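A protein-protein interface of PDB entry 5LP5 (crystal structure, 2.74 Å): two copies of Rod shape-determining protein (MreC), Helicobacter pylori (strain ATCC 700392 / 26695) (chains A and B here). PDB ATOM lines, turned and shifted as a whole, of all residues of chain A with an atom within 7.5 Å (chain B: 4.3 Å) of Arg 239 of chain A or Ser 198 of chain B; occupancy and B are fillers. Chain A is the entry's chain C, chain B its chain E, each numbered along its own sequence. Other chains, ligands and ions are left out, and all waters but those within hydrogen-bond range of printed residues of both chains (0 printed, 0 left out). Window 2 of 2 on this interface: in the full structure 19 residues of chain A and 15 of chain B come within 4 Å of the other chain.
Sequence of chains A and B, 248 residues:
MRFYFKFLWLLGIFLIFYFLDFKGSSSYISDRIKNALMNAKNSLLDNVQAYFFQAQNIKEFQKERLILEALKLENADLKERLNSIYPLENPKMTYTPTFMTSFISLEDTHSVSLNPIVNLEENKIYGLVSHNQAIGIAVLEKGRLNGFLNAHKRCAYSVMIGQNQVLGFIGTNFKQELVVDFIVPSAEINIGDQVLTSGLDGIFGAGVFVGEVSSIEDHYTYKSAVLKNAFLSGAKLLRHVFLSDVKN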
ATOM      1  N   THR A  98      24.450  -8.936 -21.305  1.00  0.00           N
ATOM      2  CA  THR A  98      24.963  -7.755 -21.985  1.00  0.00           C
ATOM      3  C   THR A  98      23.749  -6.915 -22.263  1.00  0.00           C
ATOM      4  O   THR A  98      22.607  -7.447 -22.246  1.00  0.00           O
ATOM      5  CB  THR A  98      25.692  -8.102 -23.326  1.00  0.00           C
ATOM      6  OG1 THR A  98      26.206  -6.906 -23.952  1.00  0.00           O
ATOM      7  CG2 THR A  98      24.760  -8.825 -24.311  1.00  0.00           C
ATOM      8  N   PHE A  99      23.971  -5.630 -22.523  1.00  0.00           N
ATOM      9  CA  PHE A  99      22.853  -4.810 -22.901  1.00  0.00           C
ATOM     10  C   PHE A  99      23.271  -3.736 -23.856  1.00  0.00           C
ATOM     11  O   PHE A  99      24.432  -3.374 -23.893  1.00  0.00           O
ATOM     12  CB  PHE A  99      22.180  -4.205 -21.661  1.00  0.00           C
ATOM     13  CG  PHE A  99      23.097  -3.391 -20.811  1.00  0.00           C
ATOM     14  CD1 PHE A  99      23.072  -2.018 -20.936  1.00  0.00           C
ATOM     15  CD2 PHE A  99      23.993  -3.973 -19.911  1.00  0.00           C
ATOM     16  CE1 PHE A  99      23.889  -1.209 -20.154  1.00  0.00           C
ATOM     17  CE2 PHE A  99      24.830  -3.169 -19.143  1.00  0.00           C
ATOM     18  CZ  PHE A  99      24.764  -1.786 -19.254  1.00  0.00           C
ATOM     19  N   MET A 100      22.302  -3.248 -24.629  1.00  0.00           N
ATOM     20  CA  MET A 100      22.588  -2.233 -25.628  1.00  0.00           C
ATOM     21  C   MET A 100      22.531  -0.850 -24.997  1.00  0.00           C
ATOM     22  O   MET A 100      21.685  -0.565 -24.175  1.00  0.00           O
ATOM     23  CB  MET A 100      21.680  -2.367 -26.858  1.00  0.00           C
ATOM     24  CG  MET A 100      20.281  -1.825 -26.718  1.00  0.00           C
ATOM     25  SD  MET A 100      19.306  -2.152 -28.196  1.00  0.00           S
ATOM     26  CE  MET A 100      19.742  -0.739 -29.214  1.00  0.00           C
ATOM     27  N   PHE A 103      21.622   2.396 -30.554  1.00  0.00           N
ATOM     28  CA  PHE A 103      21.838   1.883 -31.910  1.00  0.00           C
ATOM     29  C   PHE A 103      23.130   2.513 -32.428  1.00  0.00           C
ATOM     30  O   PHE A 103      23.526   3.577 -31.955  1.00  0.00           O
ATOM     31  CB  PHE A 103      20.687   2.268 -32.803  1.00  0.00           C
ATOM     32  CG  PHE A 103      19.405   1.600 -32.448  1.00  0.00           C
ATOM     33  CD1 PHE A 103      19.033   0.403 -33.034  1.00  0.00           C
ATOM     34  CD2 PHE A 103      18.530   2.201 -31.555  1.00  0.00           C
ATOM     35  CE1 PHE A 103      17.821  -0.177 -32.708  1.00  0.00           C
ATOM     36  CE2 PHE A 103      17.324   1.616 -31.221  1.00  0.00           C
ATOM     37  CZ  PHE A 103      16.969   0.426 -31.797  1.00  0.00           C
ATOM     38  N   VAL A 129      21.479 -13.888 -27.897  1.00  0.00           N
ATOM     39  CA  VAL A 129      20.253 -14.596 -27.560  1.00  0.00           C
ATOM     40  C   VAL A 129      19.419 -13.693 -26.666  1.00  0.00           C
ATOM     41  O   VAL A 129      19.969 -13.032 -25.792  1.00  0.00           O
ATOM     42  CB  VAL A 129      20.595 -15.898 -26.789  1.00  0.00           C
ATOM     43  CG1 VAL A 129      19.346 -16.642 -26.350  1.00  0.00           C
ATOM     44  CG2 VAL A 129      21.425 -16.805 -27.665  1.00  0.00           C
ATOM     45  N   SER A 130      18.099 -13.668 -26.885  1.00  0.00           N
ATOM     46  CA  SER A 130      17.211 -12.963 -25.978  1.00  0.00           C
ATOM     47  C   SER A 130      16.191 -13.876 -25.312  1.00  0.00           C
ATOM     48  O   SER A 130      16.478 -14.471 -24.262  1.00  0.00           O
ATOM     49  CB  SER A 130      16.573 -11.726 -26.593  1.00  0.00           C
ATOM     50  OG  SER A 130      15.981 -10.928 -25.570  1.00  0.00           O
ATOM     51  N   HIS A 131      14.997 -13.978 -25.853  1.00  0.00           N
ATOM     52  CA  HIS A 131      13.965 -14.718 -25.127  1.00  0.00           C
ATOM     53  C   HIS A 131      14.017 -16.135 -25.628  1.00  0.00           C
ATOM     54  O   HIS A 131      13.133 -16.578 -26.347  1.00  0.00           O
ATOM     55  CB  HIS A 131      12.594 -14.082 -25.321  1.00  0.00           C
ATOM     56  CG  HIS A 131      12.403 -12.822 -24.538  1.00  0.00           C
ATOM     57  ND1 HIS A 131      13.324 -11.795 -24.531  1.00  0.00           N
ATOM     58  CD2 HIS A 131      11.383 -12.419 -23.739  1.00  0.00           C
ATOM     59  CE1 HIS A 131      12.886 -10.823 -23.746  1.00  0.00           C
ATOM     60  NE2 HIS A 131      11.711 -11.176 -23.253  1.00  0.00           N
ATOM     61  N   ILE A 135      18.953 -13.690 -31.899  1.00  0.00           N
ATOM     62  CA  ILE A 135      18.686 -12.343 -32.462  1.00  0.00           C
ATOM     63  C   ILE A 135      19.783 -11.821 -33.375  1.00  0.00           C
ATOM     64  O   ILE A 135      19.541 -10.913 -34.155  1.00  0.00           O
ATOM     65  CB  ILE A 135      18.411 -11.273 -31.376  1.00  0.00           C
ATOM     66  CG1 ILE A 135      19.645 -11.051 -30.470  1.00  0.00           C
ATOM     67  CG2 ILE A 135      17.213 -11.684 -30.546  1.00  0.00           C
ATOM     68  CD1 ILE A 135      19.509  -9.864 -29.528  1.00  0.00           C
ATOM     69  N   GLY A 234      11.624  -6.378 -33.324  1.00  0.00           N
ATOM     70  CA  GLY A 234      10.793  -6.412 -32.112  1.00  0.00           C
ATOM     71  C   GLY A 234      11.497  -5.974 -30.837  1.00  0.00           C
ATOM     72  O   GLY A 234      12.422  -6.642 -30.382  1.00  0.00           O
ATOM     73  N   ALA A 235      11.022  -4.888 -30.234  1.00  0.00           N
ATOM     74  CA  ALA A 235      11.753  -4.221 -29.168  1.00  0.00           C
ATOM     75  C   ALA A 235      11.835  -4.985 -27.854  1.00  0.00           C
ATOM     76  O   ALA A 235      12.710  -4.692 -27.030  1.00  0.00           O
ATOM     77  CB  ALA A 235      11.166  -2.848 -28.910  1.00  0.00           C
ATOM     78  N   LYS A 236      10.942  -5.950 -27.648  1.00  0.00           N
ATOM     79  CA  LYS A 236      10.943  -6.686 -26.396  1.00  0.00           C
ATOM     80  C   LYS A 236      12.219  -7.489 -26.221  1.00  0.00           C
ATOM     81  O   LYS A 236      12.714  -7.580 -25.116  1.00  0.00           O
ATOM     82  CB  LYS A 236       9.710  -7.570 -26.268  1.00  0.00           C
ATOM     83  CG  LYS A 236       8.614  -6.924 -25.435  1.00  0.00           C
ATOM     84  CD  LYS A 236       7.277  -7.646 -25.581  1.00  0.00           C
ATOM     85  CE  LYS A 236       6.263  -7.242 -24.510  1.00  0.00           C
ATOM     86  NZ  LYS A 236       5.313  -8.359 -24.226  1.00  0.00           N
ATOM     87  N   LEU A 237      12.750  -8.019 -27.324  1.00  0.00           N
ATOM     88  CA  LEU A 237      13.916  -8.906 -27.301  1.00  0.00           C
ATOM     89  C   LEU A 237      15.260  -8.198 -27.397  1.00  0.00           C
ATOM     90  O   LEU A 237      16.280  -8.869 -27.533  1.00  0.00           O
ATOM     91  CB  LEU A 237      13.811  -9.949 -28.430  1.00  0.00           C
ATOM     92  CG  LEU A 237      13.050 -11.239 -28.070  1.00  0.00           C
ATOM     93  CD1 LEU A 237      11.571 -10.995 -27.859  1.00  0.00           C
ATOM     94  CD2 LEU A 237      13.259 -12.304 -29.138  1.00  0.00           C
ATOM     95  N   LEU A 238      15.277  -6.866 -27.379  1.00  0.00           N
ATOM     96  CA  LEU A 238      16.541  -6.154 -27.347  1.00  0.00           C
ATOM     97  C   LEU A 238      16.944  -5.867 -25.909  1.00  0.00           C
ATOM     98  O   LEU A 238      18.063  -5.439 -25.633  1.00  0.00           O
ATOM     99  CB  LEU A 238      16.503  -4.930 -28.259  1.00  0.00           C
ATOM    100  CG  LEU A 238      16.750  -5.274 -29.742  1.00  0.00           C
ATOM    101  CD1 LEU A 238      16.623  -4.060 -30.654  1.00  0.00           C
ATOM    102  CD2 LEU A 238      18.112  -5.921 -29.977  1.00  0.00           C
ATOM    103  N   ARG A 239      16.034  -6.136 -24.975  1.00  0.00           N
ATOM    104  CA  ARG A 239      16.400  -6.194 -23.559  1.00  0.00           C
ATOM    105  C   ARG A 239      16.471  -7.645 -23.109  1.00  0.00           C
ATOM    106  O   ARG A 239      15.910  -8.531 -23.745  1.00  0.00           O
ATOM    107  CB  ARG A 239      15.437  -5.373 -22.708  1.00  0.00           C
ATOM    108  CG  ARG A 239      15.621  -3.872 -22.962  1.00  0.00           C
ATOM    109  CD  ARG A 239      14.779  -2.971 -22.085  1.00  0.00           C
ATOM    110  NE  ARG A 239      13.375  -3.404 -21.979  1.00  0.00           N
ATOM    111  CZ  ARG A 239      12.374  -3.038 -22.786  1.00  0.00           C
ATOM    112  NH1 ARG A 239      12.577  -2.235 -23.821  1.00  0.00           N
ATOM    113  NH2 ARG A 239      11.152  -3.501 -22.550  1.00  0.00           N
ATOM    114  N   HIS A 240      17.192  -7.873 -22.014  1.00  0.00           N
ATOM    115  CA  HIS A 240      17.435  -9.215 -21.467  1.00  0.00           C
ATOM    116  C   HIS A 240      18.292 -10.082 -22.388  1.00  0.00           C
ATOM    117  O   HIS A 240      17.929 -11.225 -22.665  1.00  0.00           O
ATOM    118  CB  HIS A 240      16.123  -9.930 -21.143  1.00  0.00           C
ATOM    119  CG  HIS A 240      15.288  -9.233 -20.113  1.00  0.00           C
ATOM    120  ND1 HIS A 240      15.743  -8.970 -18.834  1.00  0.00           N
ATOM    121  CD2 HIS A 240      14.012  -8.775 -20.161  1.00  0.00           C
ATOM    122  CE1 HIS A 240      14.794  -8.353 -18.151  1.00  0.00           C
ATOM    123  NE2 HIS A 240      13.734  -8.226 -18.930  1.00  0.00           N
ATOM    124  N   VAL A 241      19.421  -9.526 -22.840  1.00  0.00           N
ATOM    125  CA  VAL A 241      20.234 -10.135 -23.883  1.00  0.00           C
ATOM    126  C   VAL A 241      21.471 -10.801 -23.310  1.00  0.00           C
ATOM    127  O   VAL A 241      22.137 -10.228 -22.454  1.00  0.00           O
ATOM    128  CB  VAL A 241      20.669  -9.108 -24.937  1.00  0.00           C
ATOM    129  CG1 VAL A 241      21.601  -9.742 -25.968  1.00  0.00           C
ATOM    130  CG2 VAL A 241      19.451  -8.490 -25.609  1.00  0.00           C
ATOM    131  N   PHE A 242      21.755 -12.010 -23.799  1.00  0.00           N
ATOM    132  CA  PHE A 242      22.904 -12.799 -23.371  1.00  0.00           C
ATOM    133  C   PHE A 242      23.867 -13.048 -24.540  1.00  0.00           C
ATOM    134  O   PHE A 242      23.446 -13.342 -25.649  1.00  0.00           O
ATOM    135  CB  PHE A 242      22.418 -14.139 -22.819  1.00  0.00           C
ATOM    136  CG  PHE A 242      21.657 -14.027 -21.534  1.00  0.00           C
ATOM    137  CD1 PHE A 242      22.312 -14.118 -20.322  1.00  0.00           C
ATOM    138  CD2 PHE A 242      20.290 -13.880 -21.530  1.00  0.00           C
ATOM    139  CE1 PHE A 242      21.619 -14.028 -19.128  1.00  0.00           C
ATOM    140  CE2 PHE A 242      19.580 -13.783 -20.336  1.00  0.00           C
ATOM    141  CZ  PHE A 242      20.249 -13.857 -19.135  1.00  0.00           C
ATOM    142  N   SER B 158      14.478   6.727 -31.344  1.00  0.00           N
ATOM    143  CA  SER B 158      13.890   5.391 -31.487  1.00  0.00           C
ATOM    144  C   SER B 158      12.534   5.228 -30.835  1.00  0.00           C
ATOM    145  O   SER B 158      12.360   5.527 -29.655  1.00  0.00           O
ATOM    146  CB  SER B 158      14.803   4.320 -30.921  1.00  0.00           C
ATOM    147  OG  SER B 158      14.301   3.031 -31.210  1.00  0.00           O
ATOM    148  N   VAL B 159      11.585   4.723 -31.616  1.00  0.00           N
ATOM    149  CA  VAL B 159      10.229   4.517 -31.148  1.00  0.00           C
ATOM    150  C   VAL B 159       9.796   3.084 -31.451  1.00  0.00           C
ATOM    151  O   VAL B 159      10.408   2.365 -32.269  1.00  0.00           O
ATOM    152  CB  VAL B 159       9.246   5.498 -31.792  1.00  0.00           C
ATOM    153  CG1 VAL B 159       9.606   6.913 -31.424  1.00  0.00           C
ATOM    154  CG2 VAL B 159       9.200   5.342 -33.314  1.00  0.00           C
ATOM    155  N   MET B 160       8.728   2.674 -30.777  1.00  0.00           N
ATOM    156  CA  MET B 160       8.145   1.340 -30.970  1.00  0.00           C
ATOM    157  C   MET B 160       6.636   1.431 -31.182  1.00  0.00           C
ATOM    158  O   MET B 160       5.962   2.228 -30.550  1.00  0.00           O
ATOM    159  CB  MET B 160       8.496   0.428 -29.800  1.00  0.00           C
ATOM    160  CG  MET B 160       7.996   0.900 -28.449  1.00  0.00           C
ATOM    161  SD  MET B 160       8.708  -0.153 -27.157  1.00  0.00           S
ATOM    162  CE  MET B 160       7.994   0.587 -25.699  1.00  0.00           C
ATOM    163  N   LEU B 167       9.924  -1.699 -34.167  1.00  0.00           N
ATOM    164  CA  LEU B 167      10.890  -0.606 -34.121  1.00  0.00           C
ATOM    165  C   LEU B 167      10.973   0.209 -35.396  1.00  0.00           C
ATOM    166  O   LEU B 167      10.841  -0.313 -36.515  1.00  0.00           O
ATOM    167  CB  LEU B 167      12.283  -1.164 -33.808  1.00  0.00           C
ATOM    168  CG  LEU B 167      12.464  -1.667 -32.378  1.00  0.00           C
ATOM    169  CD1 LEU B 167      13.788  -2.401 -32.246  1.00  0.00           C
ATOM    170  CD2 LEU B 167      12.385  -0.509 -31.392  1.00  0.00           C
ATOM    171  N   LEU B 196       5.246   4.719 -29.068  1.00  0.00           N
ATOM    172  CA  LEU B 196       5.931   5.096 -27.832  1.00  0.00           C
ATOM    173  C   LEU B 196       7.429   5.109 -28.042  1.00  0.00           C
ATOM    174  O   LEU B 196       7.946   4.427 -28.918  1.00  0.00           O
ATOM    175  CB  LEU B 196       5.626   4.093 -26.732  1.00  0.00           C
ATOM    176  CG  LEU B 196       4.155   3.900 -26.408  1.00  0.00           C
ATOM    177  CD1 LEU B 196       3.949   2.726 -25.466  1.00  0.00           C
ATOM    178  CD2 LEU B 196       3.563   5.155 -25.814  1.00  0.00           C
ATOM    179  N   THR B 197       8.145   5.880 -27.239  1.00  0.00           N
ATOM    180  CA  THR B 197       9.592   5.817 -27.273  1.00  0.00           C
ATOM    181  C   THR B 197      10.019   4.400 -26.888  1.00  0.00           C
ATOM    182  O   THR B 197       9.465   3.806 -25.948  1.00  0.00           O
ATOM    183  CB  THR B 197      10.240   6.815 -26.312  1.00  0.00           C
ATOM    184  OG1 THR B 197       9.846   6.535 -24.974  1.00  0.00           O
ATOM    185  CG2 THR B 197       9.835   8.220 -26.688  1.00  0.00           C
ATOM    186  N   SER B 198      11.014   3.864 -27.601  1.00  0.00           N
ATOM    187  CA  SER B 198      11.454   2.493 -27.386  1.00  0.00           C
ATOM    188  C   SER B 198      12.330   2.373 -26.152  1.00  0.00           C
ATOM    189  O   SER B 198      12.404   1.335 -25.540  1.00  0.00           O
ATOM    190  CB  SER B 198      12.235   1.999 -28.606  1.00  0.00           C
ATOM    191  OG  SER B 198      13.613   2.347 -28.507  1.00  0.00           O
ATOM    192  N   GLY B 199      13.021   3.445 -25.822  1.00  0.00           N
ATOM    193  CA  GLY B 199      13.906   3.446 -24.692  1.00  0.00           C
ATOM    194  C   GLY B 199      15.153   2.634 -24.892  1.00  0.00           C
ATOM    195  O   GLY B 199      15.792   2.276 -23.913  1.00  0.00           O
ATOM    196  N   LEU B 200      15.517   2.358 -26.141  1.00  0.00           N
ATOM    197  CA  LEU B 200      16.754   1.634 -26.400  1.00  0.00           C
ATOM    198  C   LEU B 200      17.881   2.528 -26.909  1.00  0.00           C
ATOM    199  O   LEU B 200      19.033   2.084 -27.001  1.00  0.00           O
ATOM    200  CB  LEU B 200      16.553   0.503 -27.397  1.00  0.00           C
ATOM    201  CG  LEU B 200      15.336  -0.417 -27.281  1.00  0.00           C
ATOM    202  CD1 LEU B 200      14.870  -0.921 -28.646  1.00  0.00           C
ATOM    203  CD2 LEU B 200      15.636  -1.566 -26.361  1.00  0.00           C
ATOM    204  N   ALA B 206      11.779   4.121 -21.965  1.00  0.00           N
ATOM    205  CA  ALA B 206      10.705   3.478 -22.710  1.00  0.00           C
ATOM    206  C   ALA B 206       9.339   3.986 -22.298  1.00  0.00           C
ATOM    207  O   ALA B 206       9.109   4.355 -21.145  1.00  0.00           O
ATOM    208  CB  ALA B 206      10.750   1.977 -22.525  1.00  0.00           C
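Of the 10 printed residues of chain B, 4 touch a printed residue of chain A. Hydrophobic or aromatic side chains of chain A that line the printed part of chain B: Met 100, Phe 103, Ala 235 and Leu 238. Among the printed residues, 6 pairs touch across the chains. Among the printed residues, no Asp or Glu carboxylate lies within 4 Å of a Lys or Arg side-chain nitrogen of the other chain.
Arg 239 of chain A touches just one residue of chain B: Ser 198 (3.97 Å). Of chain A, only Arg 239 (3.97 Å) comes within 4 Å of Ser 198 of chain B. Of the printed residues of chain A, Leu 167 of chain B touches Ala 235 and Leu 238. Of the printed residues of chain B, Phe 103 of chain A touches Ser 158 (3.3 Å). Of the printed residues of chain B, Met 100 of chain A touches Leu 200 (3.7 Å). Printed residues of chain B within 4 Å of Ala 235 of chain A: Leu 167. Printed residues of chain B within 4 Å of Leu 238 of chain A: Leu 167 (3.7 Å) and Leu 200 (3.96 Å). Val 241 of chain A touches none of the printed residues of chain B. The nearest residue of chain B that does not touch Arg 239 of chain A is Leu 200 of chain B (4.03 Å). The nearest printed residue of chain A that does not touch Leu 200 of chain B is Phe 103 of chain A (4.02 Å).
No position is printed for both chains. Of the 6 pairs that touch across the chains among the printed residues, none has its exchanged pair printed and touching as well.
O of Arg 239 of chain A lies within hydrogen-bond range of OG of Ser 130 of chain A, 3.0 Å away. OG of Ser 158 of chain B is in hydrogen-bond range of OG of Ser 198 of chain B, at 2.9 Å. The backbone NH (N) of Leu 200 of chain B sits at hydrogen-bond distance from the side-chain hydroxyl (OG) of Ser 198 of chain B, at 3.0 Å.
Among the printed residues, pairs that only touch across the chains: Phe 103 of chain A with Ser 158 of chain B, Ala 235 of chain A with Leu 167 of chain B, Leu 238 of chain A with Leu 167 of chain B, Met 100 of chain A with Leu 200 of chain B, Leu 238 of chain A with Leu 200 of chain B and Arg 239 of chain A with Ser 198 of chain B.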
